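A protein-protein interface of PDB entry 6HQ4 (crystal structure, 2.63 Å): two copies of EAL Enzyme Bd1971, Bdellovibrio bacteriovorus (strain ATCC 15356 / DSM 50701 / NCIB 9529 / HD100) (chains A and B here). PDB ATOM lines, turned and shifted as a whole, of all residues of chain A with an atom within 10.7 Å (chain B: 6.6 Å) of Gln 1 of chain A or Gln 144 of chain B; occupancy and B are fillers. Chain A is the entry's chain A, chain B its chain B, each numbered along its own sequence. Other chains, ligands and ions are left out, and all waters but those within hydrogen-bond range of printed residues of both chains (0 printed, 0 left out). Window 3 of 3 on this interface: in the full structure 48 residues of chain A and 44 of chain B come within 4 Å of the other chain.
Gln 1 of chain A touches just these residues of chain B: Lys 140 (3.4 Å) and Gln 144 (3.9 Å).
Gln 144 of chain B touches just one residue of chain A: Gln 1.
Leu 141 of chain B touches none of the printed residues of chain A.
Ala 148 of chain B touches none of the printed residues of chain A.
Printed residues of chain A within 4 Å of Glu 142 of chain B: Gln 81 (3.4 Å) and Arg 85 (2.5 Å).
Of the printed residues of chain B, Glu 25 of chain A touches Lys 140 (2.8 Å).
Phe 149 of chain B touches none of the printed residues of chain A.
The nearest residue of chain A that does not touch Gln 144 of chain B is Gln 81 of chain A (6.8 Å).
No position is printed for both chains.
Of the 11 pairs that touch across the chains among the printed residues, none has its exchanged pair printed and touching as well.
The backbone carbonyl oxygen (O) of Lys 140 of chain B sits at hydrogen-bond distance from the side-chain amide nitrogen (NE2) of Gln 1 of chain A (3.4 Å).
NZ of Lys 140 of chain B is in salt-bridge range of OE2 of Glu 25 of chain A (2.8 Å).
The backbone carbonyl oxygen (O) of Ile 76 of chain A is in hydrogen-bond range of the side-chain amide nitrogen (ND2) of Asn 143 of chain B (3.2 Å).
The side-chain amide nitrogen of Gln 81 of chain A is in hydrogen-bond range of the backbone carbonyl oxygen of Ile 139 of chain B (2.9 Å).
The side-chain amide nitrogen (NE2) of Gln 81 of chain A is in hydrogen-bond range of the side-chain carboxylate (OE1) of Glu 142 of chain B (3.4 Å).
OE1 of Gln 81 of chain A is in hydrogen-bond range of ND2 of Asn 143 of chain B.
The guanidinium group (NH2) of Arg 85 of chain A lies within salt-bridge range of the side-chain carboxylate (OE1) of Glu 142 of chain B, at 2.5 Å.
Printed residues of chain A that touch a printed residue of chain B: Gln 1, Ile 23, Glu 25, Ile 76, Val 77, Gln 81 and Arg 85.
Hydrophobic or aromatic side chains of chain A that line the printed part of chain B: Ile 23 and Val 77.
The backbone carbonyl oxygen (O) of Gln 1 of chain A is in hydrogen-bond range of the backbone NH (N) of Ile 76 of chain A (3.3 Å).
The side-chain hydroxyl of Ser 2 of chain A lies within hydrogen-bond range of the side-chain carboxylate of Glu 25 of chain A (3.1 Å).
The backbone carbonyl oxygen (O) of Val 77 of chain A lies within hydrogen-bond range of the backbone NH (N) of Ala 21 of chain A.
N of Thr 78 of chain A sits at hydrogen-bond distance from OE1 of Gln 81 of chain A.
O of Gln 81 of chain A sits at hydrogen-bond distance from NH1 of Arg 85 of chain A (3.0 Å).
The backbone carbonyl oxygen (O) of Ile 139 of chain B is in hydrogen-bond range of the side-chain amide nitrogen (ND2) of Asn 143 of chain B (3.4 Å).
NE2 of Gln 1 of chain A touches CB of Gln 144 of chain B, at 3.9 Å.
Ile 23 of chain A touches Ile 139 of chain B.
CG2 of Ile 139 of chain B touches O of Ile 76 of chain A, at 3.9 Å.
Val 77 of chain A touches Ile 139 of chain B.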
ATOM      1  N   GLN A   1      17.796  -0.975  20.250  1.00  0.00           N
ATOM      2  CA  GLN A   1      18.775  -0.636  19.170  1.00  0.00           C
ATOM      3  C   GLN A   1      18.204   0.332  18.130  1.00  0.00           C
ATOM      4  O   GLN A   1      18.917   1.211  17.649  1.00  0.00           O
ATOM      5  CB  GLN A   1      19.305  -1.913  18.508  1.00  0.00           C
ATOM      6  CG  GLN A   1      18.329  -2.686  17.629  1.00  0.00           C
ATOM      7  CD  GLN A   1      18.913  -4.005  17.132  1.00  0.00           C
ATOM      8  OE1 GLN A   1      18.348  -5.073  17.375  1.00  0.00           O
ATOM      9  NE2 GLN A   1      20.050  -3.935  16.444  1.00  0.00           N
ATOM     10  N   SER A   2      16.934   0.144  17.769  1.00  0.00           N
ATOM     11  CA  SER A   2      16.169   1.141  17.021  1.00  0.00           C
ATOM     12  C   SER A   2      15.173   1.816  17.974  1.00  0.00           C
ATOM     13  O   SER A   2      14.696   1.187  18.921  1.00  0.00           O
ATOM     14  CB  SER A   2      15.447   0.483  15.846  1.00  0.00           C
ATOM     15  OG  SER A   2      14.718   1.433  15.098  1.00  0.00           O
ATOM     16  N   VAL A   3      14.866   3.088  17.715  1.00  0.00           N
ATOM     17  CA  VAL A   3      14.083   3.923  18.641  1.00  0.00           C
ATOM     18  C   VAL A   3      12.985   4.718  17.931  1.00  0.00           C
ATOM     19  O   VAL A   3      13.244   5.342  16.906  1.00  0.00           O
ATOM     20  CB  VAL A   3      15.001   4.931  19.370  1.00  0.00           C
ATOM     21  CG1 VAL A   3      14.186   5.915  20.204  1.00  0.00           C
ATOM     22  CG2 VAL A   3      16.012   4.193  20.237  1.00  0.00           C
ATOM     23  N   ASP A   4      11.775   4.709  18.494  1.00  0.00           N
ATOM     24  CA  ASP A   4      10.649   5.491  17.968  1.00  0.00           C
ATOM     25  C   ASP A   4      10.604   6.880  18.603  1.00  0.00           C
ATOM     26  O   ASP A   4      10.916   7.040  19.787  1.00  0.00           O
ATOM     27  CB  ASP A   4       9.316   4.771  18.210  1.00  0.00           C
ATOM     28  CG  ASP A   4       9.116   3.576  17.292  1.00  0.00           C
ATOM     29  OD1 ASP A   4       9.447   3.668  16.090  1.00  0.00           O
ATOM     30  OD2 ASP A   4       8.614   2.538  17.777  1.00  0.00           O
ATOM     31  N   CYS A  20      25.497  10.550  21.325  1.00  0.00           N
ATOM     32  CA  CYS A  20      25.457   9.627  20.185  1.00  0.00           C
ATOM     33  C   CYS A  20      24.946  10.278  18.886  1.00  0.00           C
ATOM     34  O   CYS A  20      24.608  11.462  18.861  1.00  0.00           O
ATOM     35  CB  CYS A  20      24.594   8.416  20.544  1.00  0.00           C
ATOM     36  SG  CYS A  20      22.847   8.801  20.773  1.00  0.00           S
ATOM     37  N   ALA A  21      24.919   9.491  17.812  1.00  0.00           N
ATOM     38  CA  ALA A  21      24.400   9.918  16.512  1.00  0.00           C
ATOM     39  C   ALA A  21      23.292   8.968  16.060  1.00  0.00           C
ATOM     40  O   ALA A  21      23.087   7.920  16.667  1.00  0.00           O
ATOM     41  CB  ALA A  21      25.517   9.948  15.484  1.00  0.00           C
ATOM     42  N   TYR A  22      22.587   9.335  14.993  1.00  0.00           N
ATOM     43  CA  TYR A  22      21.408   8.587  14.551  1.00  0.00           C
ATOM     44  C   TYR A  22      21.362   8.403  13.044  1.00  0.00           C
ATOM     45  O   TYR A  22      21.882   9.228  12.300  1.00  0.00           O
ATOM     46  CB  TYR A  22      20.136   9.297  15.012  1.00  0.00           C
ATOM     47  CG  TYR A  22      20.113   9.568  16.498  1.00  0.00           C
ATOM     48  CD1 TYR A  22      19.612   8.626  17.392  1.00  0.00           C
ATOM     49  CD2 TYR A  22      20.608  10.761  17.012  1.00  0.00           C
ATOM     50  CE1 TYR A  22      19.596   8.870  18.755  1.00  0.00           C
ATOM     51  CE2 TYR A  22      20.595  11.013  18.371  1.00  0.00           C
ATOM     52  CZ  TYR A  22      20.085  10.069  19.239  1.00  0.00           C
ATOM     53  OH  TYR A  22      20.081  10.319  20.592  1.00  0.00           O
ATOM     54  N   ILE A  23      20.741   7.307  12.610  1.00  0.00           N
ATOM     55  CA  ILE A  23      20.474   7.052  11.197  1.00  0.00           C
ATOM     56  C   ILE A  23      18.972   6.833  11.033  1.00  0.00           C
ATOM     57  O   ILE A  23      18.374   6.018  11.734  1.00  0.00           O
ATOM     58  CB  ILE A  23      21.233   5.813  10.681  1.00  0.00           C
ATOM     59  CG1 ILE A  23      22.748   6.040  10.768  1.00  0.00           C
ATOM     60  CG2 ILE A  23      20.827   5.502   9.247  1.00  0.00           C
ATOM     61  CD1 ILE A  23      23.577   4.781  10.625  1.00  0.00           C
ATOM     62  N   ILE A  24      18.370   7.556  10.096  1.00  0.00           N
ATOM     63  CA  ILE A  24      16.915   7.570   9.950  1.00  0.00           C
ATOM     64  C   ILE A  24      16.424   6.343   9.188  1.00  0.00           C
ATOM     65  O   ILE A  24      16.789   6.143   8.028  1.00  0.00           O
ATOM     66  CB  ILE A  24      16.441   8.843   9.217  1.00  0.00           C
ATOM     67  CG1 ILE A  24      16.846  10.097  10.003  1.00  0.00           C
ATOM     68  CG2 ILE A  24      14.932   8.815   9.010  1.00  0.00           C
ATOM     69  CD1 ILE A  24      16.849  11.368   9.179  1.00  0.00           C
ATOM     70  N   GLU A  25      15.591   5.535   9.844  1.00  0.00           N
ATOM     71  CA  GLU A  25      14.954   4.380   9.203  1.00  0.00           C
ATOM     72  C   GLU A  25      13.579   4.733   8.632  1.00  0.00           C
ATOM     73  O   GLU A  25      13.203   4.240   7.567  1.00  0.00           O
ATOM     74  CB  GLU A  25      14.831   3.220  10.189  1.00  0.00           C
ATOM     75  CG  GLU A  25      16.169   2.645  10.629  1.00  0.00           C
ATOM     76  CD  GLU A  25      16.046   1.252  11.225  1.00  0.00           C
ATOM     77  OE1 GLU A  25      15.150   1.040  12.074  1.00  0.00           O
ATOM     78  OE2 GLU A  25      16.850   0.373  10.846  1.00  0.00           O
ATOM     79  N   ARG A  73      11.585   6.725  13.242  1.00  0.00           N
ATOM     80  CA  ARG A  73      12.323   5.665  13.925  1.00  0.00           C
ATOM     81  C   ARG A  73      13.813   5.799  13.593  1.00  0.00           C
ATOM     82  O   ARG A  73      14.197   5.810  12.421  1.00  0.00           O
ATOM     83  CB  ARG A  73      11.786   4.296  13.514  1.00  0.00           C
ATOM     84  CG  ARG A  73      12.503   3.115  14.137  1.00  0.00           C
ATOM     85  CD  ARG A  73      11.664   1.851  14.052  1.00  0.00           C
ATOM     86  NE  ARG A  73      11.590   1.359  12.674  1.00  0.00           N
ATOM     87  CZ  ARG A  73      10.526   1.463  11.872  1.00  0.00           C
ATOM     88  NH1 ARG A  73       9.394   2.031  12.288  1.00  0.00           N
ATOM     89  NH2 ARG A  73      10.589   0.980  10.634  1.00  0.00           N
ATOM     90  N   LEU A  74      14.642   5.917  14.632  1.00  0.00           N
ATOM     91  CA  LEU A  74      16.087   6.145  14.476  1.00  0.00           C
ATOM     92  C   LEU A  74      16.878   4.914  14.917  1.00  0.00           C
ATOM     93  O   LEU A  74      16.505   4.245  15.885  1.00  0.00           O
ATOM     94  CB  LEU A  74      16.542   7.338  15.325  1.00  0.00           C
ATOM     95  CG  LEU A  74      16.271   8.794  14.957  1.00  0.00           C
ATOM     96  CD1 LEU A  74      15.020   8.927  14.123  1.00  0.00           C
ATOM     97  CD2 LEU A  74      16.190   9.666  16.204  1.00  0.00           C
ATOM     98  N   ALA A  75      17.973   4.635  14.207  1.00  0.00           N
ATOM     99  CA  ALA A  75      18.929   3.592  14.588  1.00  0.00           C
ATOM    100  C   ALA A  75      20.164   4.252  15.191  1.00  0.00           C
ATOM    101  O   ALA A  75      20.784   5.109  14.562  1.00  0.00           O
ATOM    102  CB  ALA A  75      19.320   2.764  13.376  1.00  0.00           C
ATOM    103  N   ILE A  76      20.522   3.845  16.405  1.00  0.00           N
ATOM    104  CA  ILE A  76      21.555   4.539  17.171  1.00  0.00           C
ATOM    105  C   ILE A  76      22.977   4.144  16.761  1.00  0.00           C
ATOM    106  O   ILE A  76      23.289   2.962  16.614  1.00  0.00           O
ATOM    107  CB  ILE A  76      21.357   4.330  18.691  1.00  0.00           C
ATOM    108  CG1 ILE A  76      19.990   4.889  19.117  1.00  0.00           C
ATOM    109  CG2 ILE A  76      22.476   5.002  19.476  1.00  0.00           C
ATOM    110  CD1 ILE A  76      19.770   4.964  20.613  1.00  0.00           C
ATOM    111  N   VAL A  77      23.822   5.158  16.576  1.00  0.00           N
ATOM    112  CA  VAL A  77      25.261   4.998  16.394  1.00  0.00           C
ATOM    113  C   VAL A  77      25.935   5.613  17.614  1.00  0.00           C
ATOM    114  O   VAL A  77      25.791   6.809  17.861  1.00  0.00           O
ATOM    115  CB  VAL A  77      25.764   5.734  15.133  1.00  0.00           C
ATOM    116  CG1 VAL A  77      27.273   5.576  14.979  1.00  0.00           C
ATOM    117  CG2 VAL A  77      25.043   5.231  13.894  1.00  0.00           C
ATOM    118  N   THR A  78      26.665   4.804  18.379  1.00  0.00           N
ATOM    119  CA  THR A  78      27.271   5.285  19.616  1.00  0.00           C
ATOM    120  C   THR A  78      28.565   6.029  19.332  1.00  0.00           C
ATOM    121  O   THR A  78      29.133   5.925  18.241  1.00  0.00           O
ATOM    122  CB  THR A  78      27.568   4.141  20.604  1.00  0.00           C
ATOM    123  OG1 THR A  78      28.614   3.313  20.088  1.00  0.00           O
ATOM    124  CG2 THR A  78      26.328   3.299  20.850  1.00  0.00           C
ATOM    125  N   GLN A  81      31.481   3.552  18.777  1.00  0.00           N
ATOM    126  CA  GLN A  81      31.480   3.011  17.415  1.00  0.00           C
ATOM    127  C   GLN A  81      32.140   3.956  16.408  1.00  0.00           C
ATOM    128  O   GLN A  81      32.885   3.509  15.531  1.00  0.00           O
ATOM    129  CB  GLN A  81      30.054   2.701  16.962  1.00  0.00           C
ATOM    130  CG  GLN A  81      29.477   1.457  17.594  1.00  0.00           C
ATOM    131  CD  GLN A  81      28.046   1.227  17.152  1.00  0.00           C
ATOM    132  OE1 GLN A  81      27.157   2.016  17.460  1.00  0.00           O
ATOM    133  NE2 GLN A  81      27.815   0.137  16.427  1.00  0.00           N
ATOM    134  N   ARG A  85      36.169   3.546  14.724  1.00  0.00           N
ATOM    135  CA  ARG A  85      36.428   3.488  13.282  1.00  0.00           C
ATOM    136  C   ARG A  85      37.307   4.640  12.784  1.00  0.00           C
ATOM    137  O   ARG A  85      38.137   4.452  11.891  1.00  0.00           O
ATOM    138  CB  ARG A  85      35.105   3.452  12.517  1.00  0.00           C
ATOM    139  CG  ARG A  85      34.363   2.136  12.672  1.00  0.00           C
ATOM    140  CD  ARG A  85      32.885   2.272  12.352  1.00  0.00           C
ATOM    141  NE  ARG A  85      32.212   0.978  12.324  1.00  0.00           N
ATOM    142  CZ  ARG A  85      31.840   0.291  13.402  1.00  0.00           C
ATOM    143  NH1 ARG A  85      32.075   0.749  14.633  1.00  0.00           N
ATOM    144  NH2 ARG A  85      31.229  -0.876  13.248  1.00  0.00           N
ATOM    145  N   ILE B 139      26.592  -1.478  11.594  1.00  0.00           N
ATOM    146  CA  ILE B 139      26.472  -0.711  12.837  1.00  0.00           C
ATOM    147  C   ILE B 139      25.485  -1.354  13.801  1.00  0.00           C
ATOM    148  O   ILE B 139      25.749  -1.416  15.005  1.00  0.00           O
ATOM    149  CB  ILE B 139      26.036   0.742  12.548  1.00  0.00           C
ATOM    150  CG1 ILE B 139      27.217   1.547  12.053  1.00  0.00           C
ATOM    151  CG2 ILE B 139      25.497   1.448  13.778  1.00  0.00           C
ATOM    152  CD1 ILE B 139      26.831   2.881  11.465  1.00  0.00           C
ATOM    153  N   LYS B 140      24.355  -1.821  13.268  1.00  0.00           N
ATOM    154  CA  LYS B 140      23.314  -2.447  14.080  1.00  0.00           C
ATOM    155  C   LYS B 140      23.748  -3.793  14.655  1.00  0.00           C
ATOM    156  O   LYS B 140      23.424  -4.100  15.796  1.00  0.00           O
ATOM    157  CB  LYS B 140      22.029  -2.629  13.270  1.00  0.00           C
ATOM    158  CG  LYS B 140      21.342  -1.325  12.897  1.00  0.00           C
ATOM    159  CD  LYS B 140      20.198  -1.570  11.916  1.00  0.00           C
ATOM    160  CE  LYS B 140      18.959  -2.064  12.645  1.00  0.00           C
ATOM    161  NZ  LYS B 140      17.771  -2.123  11.753  1.00  0.00           N
ATOM    162  N   LEU B 141      24.477  -4.591  13.873  1.00  0.00           N
ATOM    163  CA  LEU B 141      24.937  -5.904  14.340  1.00  0.00           C
ATOM    164  C   LEU B 141      25.930  -5.766  15.498  1.00  0.00           C
ATOM    165  O   LEU B 141      25.849  -6.492  16.487  1.00  0.00           O
ATOM    166  CB  LEU B 141      25.561  -6.707  13.195  1.00  0.00           C
ATOM    167  CG  LEU B 141      25.889  -8.186  13.457  1.00  0.00           C
ATOM    168  CD1 LEU B 141      24.660  -8.946  13.933  1.00  0.00           C
ATOM    169  CD2 LEU B 141      26.457  -8.841  12.204  1.00  0.00           C
ATOM    170  N   GLU B 142      26.853  -4.818  15.380  1.00  0.00           N
ATOM    171  CA  GLU B 142      27.802  -4.548  16.463  1.00  0.00           C
ATOM    172  C   GLU B 142      27.101  -4.234  17.796  1.00  0.00           C
ATOM    173  O   GLU B 142      27.537  -4.700  18.858  1.00  0.00           O
ATOM    174  CB  GLU B 142      28.736  -3.413  16.066  1.00  0.00           C
ATOM    175  CG  GLU B 142      29.962  -3.299  16.952  1.00  0.00           C
ATOM    176  CD  GLU B 142      30.813  -2.089  16.641  1.00  0.00           C
ATOM    177  OE1 GLU B 142      30.628  -1.488  15.567  1.00  0.00           O
ATOM    178  OE2 GLU B 142      31.673  -1.738  17.473  1.00  0.00           O
ATOM    179  N   ASN B 143      26.022  -3.455  17.730  1.00  0.00           N
ATOM    180  CA  ASN B 143      25.247  -3.094  18.917  1.00  0.00           C
ATOM    181  C   ASN B 143      24.344  -4.235  19.380  1.00  0.00           C
ATOM    182  O   ASN B 143      24.140  -4.413  20.575  1.00  0.00           O
ATOM    183  CB  ASN B 143      24.400  -1.838  18.656  1.00  0.00           C
ATOM    184  CG  ASN B 143      25.243  -0.589  18.465  1.00  0.00           C
ATOM    185  OD1 ASN B 143      26.344  -0.479  19.006  1.00  0.00           O
ATOM    186  ND2 ASN B 143      24.724   0.367  17.694  1.00  0.00           N
ATOM    187  N   GLN B 144      23.798  -4.985  18.427  1.00  0.00           N
ATOM    188  CA  GLN B 144      23.009  -6.176  18.717  1.00  0.00           C
ATOM    189  C   GLN B 144      23.851  -7.194  19.494  1.00  0.00           C
ATOM    190  O   GLN B 144      23.401  -7.713  20.513  1.00  0.00           O
ATOM    191  CB  GLN B 144      22.499  -6.798  17.415  1.00  0.00           C
ATOM    192  CG  GLN B 144      21.683  -8.070  17.578  1.00  0.00           C
ATOM    193  CD  GLN B 144      21.275  -8.682  16.247  1.00  0.00           C
ATOM    194  OE1 GLN B 144      21.963  -8.516  15.243  1.00  0.00           O
ATOM    195  NE2 GLN B 144      20.174  -9.427  16.245  1.00  0.00           N
ATOM    196  N   ILE B 145      25.067  -7.458  19.010  1.00  0.00           N
ATOM    197  CA  ILE B 145      26.005  -8.356  19.697  1.00  0.00           C
ATOM    198  C   ILE B 145      26.264  -7.901  21.130  1.00  0.00           C
ATOM    199  O   ILE B 145      26.198  -8.711  22.061  1.00  0.00           O
ATOM    200  CB  ILE B 145      27.357  -8.484  18.942  1.00  0.00           C
ATOM    201  CG1 ILE B 145      27.329  -9.653  17.956  1.00  0.00           C
ATOM    202  CG2 ILE B 145      28.516  -8.743  19.906  1.00  0.00           C
ATOM    203  CD1 ILE B 145      26.239  -9.603  16.912  1.00  0.00           C
ATOM    204  N   PHE B 146      26.551  -6.610  21.305  1.00  0.00           N
ATOM    205  CA  PHE B 146      26.921  -6.088  22.623  1.00  0.00           C
ATOM    206  C   PHE B 146      25.731  -6.078  23.574  1.00  0.00           C
ATOM    207  O   PHE B 146      25.896  -6.287  24.774  1.00  0.00           O
ATOM    208  CB  PHE B 146      27.539  -4.690  22.510  1.00  0.00           C
ATOM    209  CG  PHE B 146      28.205  -4.211  23.779  1.00  0.00           C
ATOM    210  CD1 PHE B 146      29.113  -5.021  24.474  1.00  0.00           C
ATOM    211  CD2 PHE B 146      27.937  -2.942  24.277  1.00  0.00           C
ATOM    212  CE1 PHE B 146      29.724  -4.576  25.641  1.00  0.00           C
ATOM    213  CE2 PHE B 146      28.545  -2.494  25.440  1.00  0.00           C
ATOM    214  CZ  PHE B 146      29.437  -3.307  26.121  1.00  0.00           C
ATOM    215  N   GLN B 147      24.535  -5.851  23.037  1.00  0.00           N
ATOM    216  CA  GLN B 147      23.315  -5.858  23.844  1.00  0.00           C
ATOM    217  C   GLN B 147      23.022  -7.276  24.314  1.00  0.00           C
ATOM    218  O   GLN B 147      22.674  -7.493  25.473  1.00  0.00           O
ATOM    219  CB  GLN B 147      22.122  -5.313  23.047  1.00  0.00           C
ATOM    220  CG  GLN B 147      20.943  -4.880  23.908  1.00  0.00           C
ATOM    221  CD  GLN B 147      19.697  -4.582  23.091  1.00  0.00           C
ATOM    222  OE1 GLN B 147      19.252  -5.411  22.295  1.00  0.00           O
ATOM    223  NE2 GLN B 147      19.120  -3.395  23.291  1.00  0.00           N
ATOM    224  N   ALA B 148      23.179  -8.234  23.403  1.00  0.00           N
ATOM    225  CA  ALA B 148      23.045  -9.652  23.731  1.00  0.00           C
ATOM    226  C   ALA B 148      24.000 -10.048  24.852  1.00  0.00           C
ATOM    227  O   ALA B 148      23.615 -10.781  25.761  1.00  0.00           O
ATOM    228  CB  ALA B 148      23.292 -10.516  22.501  1.00  0.00           C
ATOM    229  N   PHE B 149      25.235  -9.551  24.788  1.00  0.00           N
ATOM    230  CA  PHE B 149      26.219  -9.801  25.842  1.00  0.00           C
ATOM    231  C   PHE B 149      25.712  -9.328  27.203  1.00  0.00           C
ATOM    232  O   PHE B 149      25.853 -10.031  28.195  1.00  0.00           O
ATOM    233  CB  PHE B 149      27.564  -9.135  25.522  1.00  0.00           C
ATOM    234  CG  PHE B 149      28.559  -9.215  26.647  1.00  0.00           C
ATOM    235  CD1 PHE B 149      29.033 -10.450  27.082  1.00  0.00           C
ATOM    236  CD2 PHE B 149      29.013  -8.062  27.282  1.00  0.00           C
ATOM    237  CE1 PHE B 149      29.939 -10.537  28.128  1.00  0.00           C
ATOM    238  CE2 PHE B 149      29.924  -8.141  28.325  1.00  0.00           C
ATOM    239  CZ  PHE B 149      30.386  -9.381  28.749  1.00  0.00           C
ATOM    240  N   GLU B 153      23.034 -13.520  26.968  1.00  0.00           N
ATOM    241  CA  GLU B 153      22.670 -14.531  25.980  1.00  0.00           C
ATOM    242  C   GLU B 153      23.888 -15.359  25.564  1.00  0.00           C
ATOM    243  O   GLU B 153      23.747 -16.340  24.829  1.00  0.00           O
ATOM    244  CB  GLU B 153      22.025 -13.871  24.756  1.00  0.00           C
ATOM    245  CG  GLU B 153      20.739 -13.118  25.081  1.00  0.00           C
ATOM    246  CD  GLU B 153      20.209 -12.278  23.930  1.00  0.00           C
ATOM    247  OE1 GLU B 153      20.705 -12.406  22.793  1.00  0.00           O
ATOM    248  OE2 GLU B 153      19.283 -11.477  24.170  1.00  0.00           O
ATOM    249  N   PHE B 154      25.080 -14.963  26.018  1.00  0.00           N
ATOM    250  CA  PHE B 154      26.297 -15.720  25.735  1.00  0.00           C
ATOM    251  C   PHE B 154      26.574 -16.670  26.877  1.00  0.00           C
ATOM    252  O   PHE B 154      26.299 -16.357  28.033  1.00  0.00           O
ATOM    253  CB  PHE B 154      27.537 -14.820  25.586  1.00  0.00           C
ATOM    254  CG  PHE B 154      27.481 -13.839  24.443  1.00  0.00           C
ATOM    255  CD1 PHE B 154      26.474 -13.869  23.481  1.00  0.00           C
ATOM    256  CD2 PHE B 154      28.487 -12.885  24.320  1.00  0.00           C
ATOM    257  CE1 PHE B 154      26.467 -12.946  22.444  1.00  0.00           C
ATOM    258  CE2 PHE B 154      28.486 -11.968  23.281  1.00  0.00           C
ATOM    259  CZ  PHE B 154      27.474 -12.000  22.338  1.00  0.00           C
ATOM    260  N   TRP B 178      26.409 -18.279  21.517  1.00  0.00           N
ATOM    261  CA  TRP B 178      25.341 -17.289  21.606  1.00  0.00           C
ATOM    262  C   TRP B 178      24.041 -17.956  21.164  1.00  0.00           C
ATOM    263  O   TRP B 178      23.919 -18.364  20.011  1.00  0.00           O
ATOM    264  CB  TRP B 178      25.632 -16.106  20.675  1.00  0.00           C
ATOM    265  CG  TRP B 178      24.564 -15.036  20.653  1.00  0.00           C
ATOM    266  CD1 TRP B 178      23.570 -14.832  21.578  1.00  0.00           C
ATOM    267  CD2 TRP B 178      24.412 -14.000  19.673  1.00  0.00           C
ATOM    268  NE1 TRP B 178      22.802 -13.755  21.221  1.00  0.00           N
ATOM    269  CE2 TRP B 178      23.298 -13.222  20.060  1.00  0.00           C
ATOM    270  CE3 TRP B 178      25.103 -13.656  18.501  1.00  0.00           C
ATOM    271  CZ2 TRP B 178      22.860 -12.126  19.321  1.00  0.00           C
ATOM    272  CZ3 TRP B 178      24.664 -12.562  17.765  1.00  0.00           C
ATOM    273  CH2 TRP B 178      23.555 -11.811  18.180  1.00  0.00           C
ATOM    274  N   SER B 180      20.317 -16.621  20.990  1.00  0.00           N
ATOM    275  CA  SER B 180      19.215 -15.677  21.163  1.00  0.00           C
ATOM    276  C   SER B 180      17.900 -16.443  21.164  1.00  0.00           C
ATOM    277  O   SER B 180      17.741 -17.390  20.393  1.00  0.00           O
ATOM    278  CB  SER B 180      19.207 -14.623  20.053  1.00  0.00           C
ATOM    279  OG  SER B 180      18.052 -13.798  20.134  1.00  0.00           O
ATOM    280  N   HIS B 183      16.304 -15.925  17.480  1.00  0.00           N
ATOM    281  CA  HIS B 183      17.039 -16.337  16.288  1.00  0.00           C
ATOM    282  C   HIS B 183      17.704 -17.688  16.547  1.00  0.00           C
ATOM    283  O   HIS B 183      18.667 -18.049  15.873  1.00  0.00           O
ATOM    284  CB  HIS B 183      18.102 -15.296  15.922  1.00  0.00           C
ATOM    285  CG  HIS B 183      17.550 -13.927  15.677  1.00  0.00           C
ATOM    286  ND1 HIS B 183      17.371 -13.002  16.682  1.00  0.00           N
ATOM    287  CD2 HIS B 183      17.142 -13.323  14.535  1.00  0.00           C
ATOM    288  CE1 HIS B 183      16.874 -11.888  16.171  1.00  0.00           C
ATOM    289  NE2 HIS B 183      16.726 -12.059  14.870  1.00  0.00           N
